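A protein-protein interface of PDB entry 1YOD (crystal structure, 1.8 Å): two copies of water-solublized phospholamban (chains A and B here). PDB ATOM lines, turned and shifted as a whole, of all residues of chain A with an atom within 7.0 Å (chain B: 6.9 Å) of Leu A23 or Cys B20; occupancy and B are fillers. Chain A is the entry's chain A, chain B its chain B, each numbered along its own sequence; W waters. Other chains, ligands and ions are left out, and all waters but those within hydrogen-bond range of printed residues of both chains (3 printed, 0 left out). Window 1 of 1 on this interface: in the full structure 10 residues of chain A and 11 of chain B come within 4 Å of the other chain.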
ATOM      1  N   LEU A  16     -10.218 -17.402  -8.531  1.00  0.00           N
ATOM      2  CA  LEU A  16      -8.783 -17.464  -8.160  1.00  0.00           C
ATOM      3  C   LEU A  16      -8.139 -16.103  -8.331  1.00  0.00           C
ATOM      4  O   LEU A  16      -7.287 -15.706  -7.530  1.00  0.00           O
ATOM      5  CB  LEU A  16      -8.031 -18.578  -8.905  1.00  0.00           C
ATOM      6  CG  LEU A  16      -8.511 -20.012  -8.679  1.00  0.00           C
ATOM      7  CD1 LEU A  16      -7.657 -21.044  -9.515  1.00  0.00           C
ATOM      8  CD2 LEU A  16      -8.516 -20.429  -7.216  1.00  0.00           C
ATOM      9  N   GLU A  18      -9.641 -13.209  -7.786  1.00  0.00           N
ATOM     10  CA  GLU A  18     -10.109 -12.475  -6.635  1.00  0.00           C
ATOM     11  C   GLU A  18      -9.316 -12.875  -5.400  1.00  0.00           C
ATOM     12  O   GLU A  18      -8.908 -12.028  -4.634  1.00  0.00           O
ATOM     13  CB  GLU A  18     -11.611 -12.625  -6.437  1.00  0.00           C
ATOM     14  CG  GLU A  18     -12.374 -11.911  -7.541  1.00  0.00           C
ATOM     15  CD  GLU A  18     -13.869 -12.253  -7.622  1.00  0.00           C
ATOM     16  OE1 GLU A  18     -14.374 -13.046  -6.809  1.00  0.00           O
ATOM     17  OE2 GLU A  18     -14.539 -11.711  -8.541  1.00  0.00           O
ATOM     18  N   ILE A  19      -9.073 -14.170  -5.234  1.00  0.00           N
ATOM     19  CA  ILE A  19      -8.263 -14.644  -4.127  1.00  0.00           C
ATOM     20  C   ILE A  19      -6.825 -14.077  -4.196  1.00  0.00           C
ATOM     21  O   ILE A  19      -6.264 -13.643  -3.169  1.00  0.00           O
ATOM     22  CB  ILE A  19      -8.274 -16.187  -4.087  1.00  0.00           C
ATOM     23  CG1 ILE A  19      -9.632 -16.685  -3.558  1.00  0.00           C
ATOM     24  CG2 ILE A  19      -7.200 -16.717  -3.217  1.00  0.00           C
ATOM     25  CD1 ILE A  19      -9.864 -18.184  -3.807  1.00  0.00           C
ATOM     26  N   CYS A  20      -6.247 -14.044  -5.378  1.00  0.00           N
ATOM     27  CA  CYS A  20      -4.894 -13.491  -5.573  1.00  0.00           C
ATOM     28  C   CYS A  20      -4.864 -12.045  -5.157  1.00  0.00           C
ATOM     29  O   CYS A  20      -3.935 -11.593  -4.460  1.00  0.00           O
ATOM     30  CB  CYS A  20      -4.461 -13.637  -7.012  1.00  0.00           C
ATOM     31  SG  CYS A  20      -3.866 -15.294  -7.426  1.00  0.00           S
ATOM     32  N   GLN A  21      -5.870 -11.298  -5.569  1.00  0.00           N
ATOM     33  CA  GLN A  21      -5.993  -9.901  -5.149  1.00  0.00           C
ATOM     34  C   GLN A  21      -6.015  -9.739  -3.624  1.00  0.00           C
ATOM     35  O   GLN A  21      -5.332  -8.874  -3.083  1.00  0.00           O
ATOM     36  CB  GLN A  21      -7.248  -9.230  -5.763  1.00  0.00           C
ATOM     37  CG  GLN A  21      -7.392  -7.741  -5.324  1.00  0.00           C
ATOM     38  CD  GLN A  21      -6.203  -6.820  -5.666  1.00  0.00           C
ATOM     39  OE1 GLN A  21      -6.025  -5.745  -5.011  1.00  0.00           O
ATOM     40  NE2 GLN A  21      -5.415  -7.191  -6.687  1.00  0.00           N
ATOM     41  N   GLU A  22      -6.808 -10.566  -2.946  1.00  0.00           N
ATOM     42  CA  GLU A  22      -6.845 -10.566  -1.508  1.00  0.00           C
ATOM     43  C   GLU A  22      -5.494 -10.895  -0.888  1.00  0.00           C
ATOM     44  O   GLU A  22      -5.077 -10.218   0.075  1.00  0.00           O
ATOM     45  CB  GLU A  22      -7.881 -11.537  -0.983  1.00  0.00           C
ATOM     46  CG  GLU A  22      -9.301 -11.221  -1.385  1.00  0.00           C
ATOM     47  CD  GLU A  22     -10.207 -12.367  -1.005  1.00  0.00           C
ATOM     48  OE1 GLU A  22     -10.467 -12.544   0.176  1.00  0.00           O
ATOM     49  OE2 GLU A  22     -10.583 -13.108  -1.899  1.00  0.00           O
ATOM     50  N   LEU A  23      -4.792 -11.901  -1.407  1.00  0.00           N
ATOM     51  CA  LEU A  23      -3.468 -12.231  -0.877  1.00  0.00           C
ATOM     52  C   LEU A  23      -2.450 -11.105  -1.102  1.00  0.00           C
ATOM     53  O   LEU A  23      -1.571 -10.859  -0.255  1.00  0.00           O
ATOM     54  CB  LEU A  23      -2.971 -13.540  -1.449  1.00  0.00           C
ATOM     55  CG  LEU A  23      -3.837 -14.759  -1.150  1.00  0.00           C
ATOM     56  CD1 LEU A  23      -3.241 -15.938  -1.867  1.00  0.00           C
ATOM     57  CD2 LEU A  23      -3.964 -15.012   0.342  1.00  0.00           C
ATOM     58  N   LYS A  24      -2.584 -10.400  -2.216  1.00  0.00           N
ATOM     59  CA  LYS A  24      -1.726  -9.214  -2.469  1.00  0.00           C
ATOM     60  C   LYS A  24      -1.971  -8.117  -1.491  1.00  0.00           C
ATOM     61  O   LYS A  24      -0.992  -7.466  -1.055  1.00  0.00           O
ATOM     62  CB  LYS A  24      -1.862  -8.722  -3.890  1.00  0.00           C
ATOM     63  CG  LYS A  24      -1.265  -9.729  -4.882  1.00  0.00           C
ATOM     64  CD  LYS A  24      -1.679  -9.305  -6.274  1.00  0.00           C
ATOM     65  CE  LYS A  24      -1.456 -10.358  -7.317  1.00  0.00           C
ATOM     66  NZ  LYS A  24      -1.406  -9.739  -8.690  1.00  0.00           N
ATOM     67  N   GLU A  25      -3.220  -7.927  -1.091  1.00  0.00           N
ATOM     68  CA  GLU A  25      -3.586  -6.957  -0.076  1.00  0.00           C
ATOM     69  C   GLU A  25      -2.997  -7.343   1.269  1.00  0.00           C
ATOM     70  O   GLU A  25      -2.421  -6.503   1.974  1.00  0.00           O
ATOM     71  CB  GLU A  25      -5.107  -6.729  -0.032  1.00  0.00           C
ATOM     72  CG  GLU A  25      -5.657  -6.104  -1.317  1.00  0.00           C
ATOM     73  CD  GLU A  25      -7.171  -6.043  -1.432  1.00  0.00           C
ATOM     74  OE1 GLU A  25      -7.880  -6.388  -0.477  1.00  0.00           O
ATOM     75  OE2 GLU A  25      -7.671  -5.619  -2.507  1.00  0.00           O
ATOM     76  N   ILE A  26      -3.071  -8.632   1.626  1.00  0.00           N
ATOM     77  CA  ILE A  26      -2.502  -9.116   2.886  1.00  0.00           C
ATOM     78  C   ILE A  26      -0.988  -8.884   2.899  1.00  0.00           C
ATOM     79  O   ILE A  26      -0.421  -8.440   3.909  1.00  0.00           O
ATOM     80  CB  ILE A  26      -2.838 -10.583   3.072  1.00  0.00           C
ATOM     81  CG1 ILE A  26      -4.305 -10.711   3.340  1.00  0.00           C
ATOM     82  CG2 ILE A  26      -2.018 -11.226   4.163  1.00  0.00           C
ATOM     83  CD1 ILE A  26      -4.846 -12.100   3.322  1.00  0.00           C
ATOM     84  N   ARG A  27      -0.327  -9.224   1.810  1.00  0.00           N
ATOM     85  CA  ARG A  27       1.130  -8.998   1.648  1.00  0.00           C
ATOM     86  C   ARG A  27       1.481  -7.550   1.899  1.00  0.00           C
ATOM     87  O   ARG A  27       2.416  -7.268   2.669  1.00  0.00           O
ATOM     88  CB  ARG A  27       1.600  -9.372   0.256  1.00  0.00           C
ATOM     89  CG  ARG A  27       1.691 -10.849   0.011  1.00  0.00           C
ATOM     90  CD  ARG A  27       1.706 -11.257  -1.450  1.00  0.00           C
ATOM     91  NE  ARG A  27       2.850 -10.732  -2.197  1.00  0.00           N
ATOM     92  CZ  ARG A  27       2.962 -10.778  -3.542  1.00  0.00           C
ATOM     93  NH1 ARG A  27       1.990 -11.288  -4.321  1.00  0.00           N
ATOM     94  NH2 ARG A  27       4.059 -10.294  -4.118  1.00  0.00           N
ATOM     95  N   ALA A  28       0.691  -6.629   1.340  1.00  0.00           N
ATOM     96  CA  ALA A  28       0.982  -5.206   1.511  1.00  0.00           C
ATOM     97  C   ALA A  28       0.835  -4.821   2.982  1.00  0.00           C
ATOM     98  O   ALA A  28       1.648  -4.039   3.512  1.00  0.00           O
ATOM     99  CB  ALA A  28       0.071  -4.383   0.667  1.00  0.00           C
ATOM    100  N   MET A  29      -0.142  -5.389   3.665  1.00  0.00           N
ATOM    101  CA  MET A  29      -0.439  -5.003   5.032  1.00  0.00           C
ATOM    102  C   MET A  29       0.647  -5.592   5.966  1.00  0.00           C
ATOM    103  O   MET A  29       1.009  -4.991   6.974  1.00  0.00           O
ATOM    104  CB  MET A  29      -1.906  -5.333   5.415  1.00  0.00           C
ATOM    105  CG  MET A  29      -3.125  -4.183   5.024  1.00  0.00           C
ATOM    106  SD  MET A  29      -4.511  -5.488   4.765  1.00  0.00           S
ATOM    107  CE  MET A  29      -4.513  -5.593   3.510  1.00  0.00           C
ATOM    108  N   ASN B  13       5.275 -13.431   3.813  1.00  0.00           N
ATOM    109  CA  ASN B  13       5.074 -12.728   2.540  1.00  0.00           C
ATOM    110  C   ASN B  13       5.699 -13.421   1.335  1.00  0.00           C
ATOM    111  O   ASN B  13       5.148 -13.380   0.254  1.00  0.00           O
ATOM    112  CB  ASN B  13       5.526 -11.264   2.622  1.00  0.00           C
ATOM    113  CG  ASN B  13       4.469 -10.362   3.239  1.00  0.00           C
ATOM    114  OD1 ASN B  13       3.327 -10.774   3.420  1.00  0.00           O
ATOM    115  ND2 ASN B  13       4.842  -9.123   3.550  1.00  0.00           N
ATOM    116  N   CYS B  15       5.951 -16.654   1.058  1.00  0.00           N
ATOM    117  CA  CYS B  15       5.069 -17.775   0.822  1.00  0.00           C
ATOM    118  C   CYS B  15       3.829 -17.271   0.084  1.00  0.00           C
ATOM    119  O   CYS B  15       3.391 -17.928  -0.829  1.00  0.00           O
ATOM    120  CB  CYS B  15       4.651 -18.516   2.081  1.00  0.00           C
ATOM    121  SG  CYS B  15       3.951 -20.173   1.727  1.00  0.00           S
ATOM    122  N   LEU B  16       3.282 -16.134   0.495  1.00  0.00           N
ATOM    123  CA  LEU B  16       2.081 -15.596  -0.157  1.00  0.00           C
ATOM    124  C   LEU B  16       2.400 -15.252  -1.592  1.00  0.00           C
ATOM    125  O   LEU B  16       1.599 -15.470  -2.461  1.00  0.00           O
ATOM    126  CB  LEU B  16       1.477 -14.419   0.606  1.00  0.00           C
ATOM    127  CG  LEU B  16       0.840 -14.741   1.953  1.00  0.00           C
ATOM    128  CD1 LEU B  16       0.475 -13.441   2.604  1.00  0.00           C
ATOM    129  CD2 LEU B  16      -0.342 -15.726   1.820  1.00  0.00           C
ATOM    130  N   ARG B  17       3.590 -14.714  -1.866  1.00  0.00           N
ATOM    131  CA  ARG B  17       3.921 -14.381  -3.232  1.00  0.00           C
ATOM    132  C   ARG B  17       4.036 -15.626  -4.071  1.00  0.00           C
ATOM    133  O   ARG B  17       3.592 -15.642  -5.200  1.00  0.00           O
ATOM    134  CB  ARG B  17       5.250 -13.631  -3.240  1.00  0.00           C
ATOM    135  CG  ARG B  17       5.853 -13.399  -4.599  1.00  0.00           C
ATOM    136  CD  ARG B  17       7.151 -12.552  -4.559  1.00  0.00           C
ATOM    137  NE  ARG B  17       7.774 -12.640  -5.870  1.00  0.00           N
ATOM    138  CZ  ARG B  17       8.792 -11.919  -6.324  1.00  0.00           C
ATOM    139  NH1 ARG B  17       9.365 -10.967  -5.587  1.00  0.00           N
ATOM    140  NH2 ARG B  17       9.225 -12.151  -7.561  1.00  0.00           N
ATOM    141  N   GLU B  18       4.601 -16.693  -3.510  1.00  0.00           N
ATOM    142  CA  GLU B  18       4.740 -17.980  -4.188  1.00  0.00           C
ATOM    143  C   GLU B  18       3.375 -18.605  -4.488  1.00  0.00           C
ATOM    144  O   GLU B  18       3.155 -19.146  -5.567  1.00  0.00           O
ATOM    145  CB  GLU B  18       5.637 -18.926  -3.360  1.00  0.00           C
ATOM    146  CG  GLU B  18       5.944 -20.263  -3.964  1.00  0.00           C
ATOM    147  CD  GLU B  18       6.959 -21.055  -3.113  1.00  0.00           C
ATOM    148  OE1 GLU B  18       8.181 -20.896  -3.355  1.00  0.00           O
ATOM    149  OE2 GLU B  18       6.534 -21.808  -2.204  1.00  0.00           O
ATOM    150  N   ILE B  19       2.448 -18.493  -3.553  1.00  0.00           N
ATOM    151  CA  ILE B  19       1.094 -18.987  -3.746  1.00  0.00           C
ATOM    152  C   ILE B  19       0.441 -18.213  -4.876  1.00  0.00           C
ATOM    153  O   ILE B  19      -0.217 -18.818  -5.715  1.00  0.00           O
ATOM    154  CB  ILE B  19       0.309 -18.849  -2.442  1.00  0.00           C
ATOM    155  CG1 ILE B  19       0.808 -19.892  -1.426  1.00  0.00           C
ATOM    156  CG2 ILE B  19      -1.180 -19.021  -2.662  1.00  0.00           C
ATOM    157  CD1 ILE B  19       0.295 -19.695  -0.027  1.00  0.00           C
ATOM    158  N   CYS B  20       0.588 -16.895  -4.858  1.00  0.00           N
ATOM    159  CA  CYS B  20       0.050 -16.067  -5.950  1.00  0.00           C
ATOM    160  C   CYS B  20       0.586 -16.485  -7.315  1.00  0.00           C
ATOM    161  O   CYS B  20      -0.178 -16.594  -8.272  1.00  0.00           O
ATOM    162  CB  CYS B  20       0.303 -14.607  -5.687  1.00  0.00           C
ATOM    163  SG  CYS B  20      -0.726 -13.921  -4.410  1.00  0.00           S
ATOM    164  N   GLN B  21       1.858 -16.826  -7.412  1.00  0.00           N
ATOM    165  CA  GLN B  21       2.426 -17.304  -8.665  1.00  0.00           C
ATOM    166  C   GLN B  21       1.864 -18.644  -9.053  1.00  0.00           C
ATOM    167  O   GLN B  21       1.615 -18.897 -10.229  1.00  0.00           O
ATOM    168  CB  GLN B  21       3.947 -17.396  -8.559  1.00  0.00           C
ATOM    169  CG  GLN B  21       4.630 -17.924  -9.827  1.00  0.00           C
ATOM    170  CD  GLN B  21       4.296 -17.147 -11.118  1.00  0.00           C
ATOM    171  OE1 GLN B  21       4.140 -17.761 -12.206  1.00  0.00           O
ATOM    172  NE2 GLN B  21       4.198 -15.828 -11.024  1.00  0.00           N
ATOM    173  N   GLU B  22       1.650 -19.535  -8.083  1.00  0.00           N
ATOM    174  CA  GLU B  22       1.064 -20.811  -8.352  1.00  0.00           C
ATOM    175  C   GLU B  22      -0.397 -20.661  -8.838  1.00  0.00           C
ATOM    176  O   GLU B  22      -0.821 -21.336  -9.798  1.00  0.00           O
ATOM    177  CB  GLU B  22       1.098 -21.686  -7.107  1.00  0.00           C
ATOM    178  CG  GLU B  22       0.570 -23.077  -7.366  1.00  0.00           C
ATOM    179  CD  GLU B  22       0.773 -24.042  -6.217  1.00  0.00           C
ATOM    180  OE1 GLU B  22       1.509 -23.677  -5.252  1.00  0.00           O
ATOM    181  OE2 GLU B  22       0.175 -25.158  -6.307  1.00  0.00           O
ATOM    182  N   LEU B  23      -1.157 -19.790  -8.190  1.00  0.00           N
ATOM    183  CA  LEU B  23      -2.549 -19.602  -8.594  1.00  0.00           C
ATOM    184  C   LEU B  23      -2.611 -18.990 -10.015  1.00  0.00           C
ATOM    185  O   LEU B  23      -3.459 -19.372 -10.802  1.00  0.00           O
ATOM    186  CB  LEU B  23      -3.263 -18.724  -7.573  1.00  0.00           C
ATOM    187  CG  LEU B  23      -3.502 -19.389  -6.203  1.00  0.00           C
ATOM    188  CD1 LEU B  23      -4.064 -18.325  -5.331  1.00  0.00           C
ATOM    189  CD2 LEU B  23      -4.445 -20.580  -6.297  1.00  0.00           C
ATOM    190  N   LYS B  24      -1.671 -18.124 -10.367  1.00  0.00           N
ATOM    191  CA  LYS B  24      -1.580 -17.582 -11.753  1.00  0.00           C
ATOM    192  C   LYS B  24      -1.307 -18.678 -12.794  1.00  0.00           C
ATOM    193  O   LYS B  24      -1.950 -18.721 -13.857  1.00  0.00           O
ATOM    194  CB  LYS B  24      -0.572 -16.431 -11.791  1.00  0.00           C
ATOM    195  CG  LYS B  24      -0.512 -15.680 -13.121  1.00  0.00           C
ATOM    196  CD  LYS B  24       0.906 -15.442 -13.578  1.00  0.00           C
ATOM    197  CE  LYS B  24       1.002 -14.265 -14.566  1.00  0.00           C
ATOM    198  NZ  LYS B  24       1.810 -13.200 -13.906  1.00  0.00           N
ATOM    199  N   GLU B  25      -0.439 -19.627 -12.466  1.00  0.00           N
ATOM    200  CA  GLU B  25      -0.207 -20.805 -13.297  1.00  0.00           C
ATOM    201  C   GLU B  25      -1.427 -21.726 -13.415  1.00  0.00           C
ATOM    202  O   GLU B  25      -1.692 -22.267 -14.497  1.00  0.00           O
ATOM    203  CB  GLU B  25       1.025 -21.585 -12.810  1.00  0.00           C
ATOM    204  CG  GLU B  25       2.287 -20.724 -12.874  1.00  0.00           C
ATOM    205  CD  GLU B  25       3.477 -21.419 -12.288  1.00  0.00           C
ATOM    206  OE1 GLU B  25       3.376 -22.641 -12.023  1.00  0.00           O
ATOM    207  OE2 GLU B  25       4.512 -20.735 -12.103  1.00  0.00           O
ATOM    208  N   ARG B  27      -4.562 -20.651 -13.113  1.00  0.00           N
ATOM    209  CA  ARG B  27      -5.513 -19.888 -13.928  1.00  0.00           C
ATOM    210  C   ARG B  27      -5.145 -20.092 -15.416  1.00  0.00           C
ATOM    211  O   ARG B  27      -6.023 -20.226 -16.254  1.00  0.00           O
ATOM    212  CB  ARG B  27      -5.494 -18.417 -13.562  1.00  0.00           C
ATOM    213  CG  ARG B  27      -6.106 -18.161 -12.187  1.00  0.00           C
ATOM    214  CD  ARG B  27      -6.067 -16.753 -11.704  1.00  0.00           C
ATOM    215  NE  ARG B  27      -6.706 -15.917 -12.679  1.00  0.00           N
ATOM    216  CZ  ARG B  27      -6.212 -14.836 -13.243  1.00  0.00           C
ATOM    217  NH1 ARG B  27      -5.040 -14.317 -12.879  1.00  0.00           N
ATOM    218  NH2 ARG B  27      -6.939 -14.222 -14.173  1.00  0.00           N
HETATM  219  O   HOH W   1      -3.572 -14.443 -10.519  1.00  0.00           O
HETATM  220  O   HOH W   2       5.214 -10.237  -1.182  1.00  0.00           O
HETATM  221  O   HOH W   3       7.053  -9.278  -4.628  1.00  0.00           O
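SG of Cys B20 lies within hydrogen-bond range of NH1 of Arg A27, 3.8 Å away. The backbone carbonyl oxygen (O) of Arg A27 sits at hydrogen-bond distance from the side-chain amide nitrogen (ND2) of Asn B13.
The backbone carbonyl oxygen (O) of Leu A16 lies within hydrogen-bond range of the side-chain sulfur (SG) of Cys A20 (3.4 Å). The side-chain sulfur of Cys B20 sits at hydrogen-bond distance from the backbone carbonyl oxygen of Leu B16.
Among the printed residues, pairs that only touch across the chains: Cys A20 with Leu B23 (3.5 Å), Arg A27 with Arg B17 (3.6 Å), Arg A27 with Leu B16 (3.6 Å), Ile A26 with Leu B16 (3.7 Å), Leu A23 with Cys B20 (3.7 Å), Leu A23 with Ile B19 (3.8 Å), Leu A16 with Arg B27 (3.8 Å), Cys A20 with Cys B20 (3.96 Å) and Leu A23 with Leu B16 (3.98 Å).
Glu A18 touches none of the printed residues of chain B. Leu A23 touches three residues of chain B. Of the printed residues of chain B, Arg A27 touches Asn B13, Leu B16, Arg B17 and Cys B20. Glu B18 touches none of the printed residues of chain A. Of chain A, only Cys A20 (3.96 Å), Leu A23 (3.7 Å) and Arg A27 (3.8 Å) come within 4 Å of Cys B20. Of the printed residues of chain A, Arg B27 touches Leu A16.
Printed residues of chain B that touch a printed residue of chain A: Asn B13, Leu B16, Arg B17, Ile B19, Cys B20, Leu B23 and Arg B27. Of the 13 printed residues of chain A, 5 touch a printed residue of chain B. Among the printed residues, 11 pairs touch across the chains. Among the printed residues, no Asp or Glu carboxylate lies within 4 Å of a Lys or Arg side-chain nitrogen of the other chain.
Cys B20 touches its own counterpart, Cys A20. Cys A20 touches Leu B23, and with the chains exchanged Leu A23 touches Cys B20. Leu A23 touches Leu B16, but with the chains exchanged Leu A16 does not touch Leu B23 (4.2 Å). Arg A27 touches Cys B20, but with the chains exchanged Cys A20 does not touch Arg B27 (5.0 Å). Of the 11 pairs that touch across the chains among the printed residues, 5 have their exchanged pair printed and touching as well.
Water W2 bridges NE of Arg A27 (2.6 Å) and O of Asn B13 (3.5 Å). Water W1 lies within hydrogen-bond range of the guanidinium group (NH1) of Arg B27 and the side-chain sulfur (SG) of Cys A20. Water W3 bridges the guanidinium group (NH1) of Arg B17 and the guanidinium group (NH2) of Arg A27.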
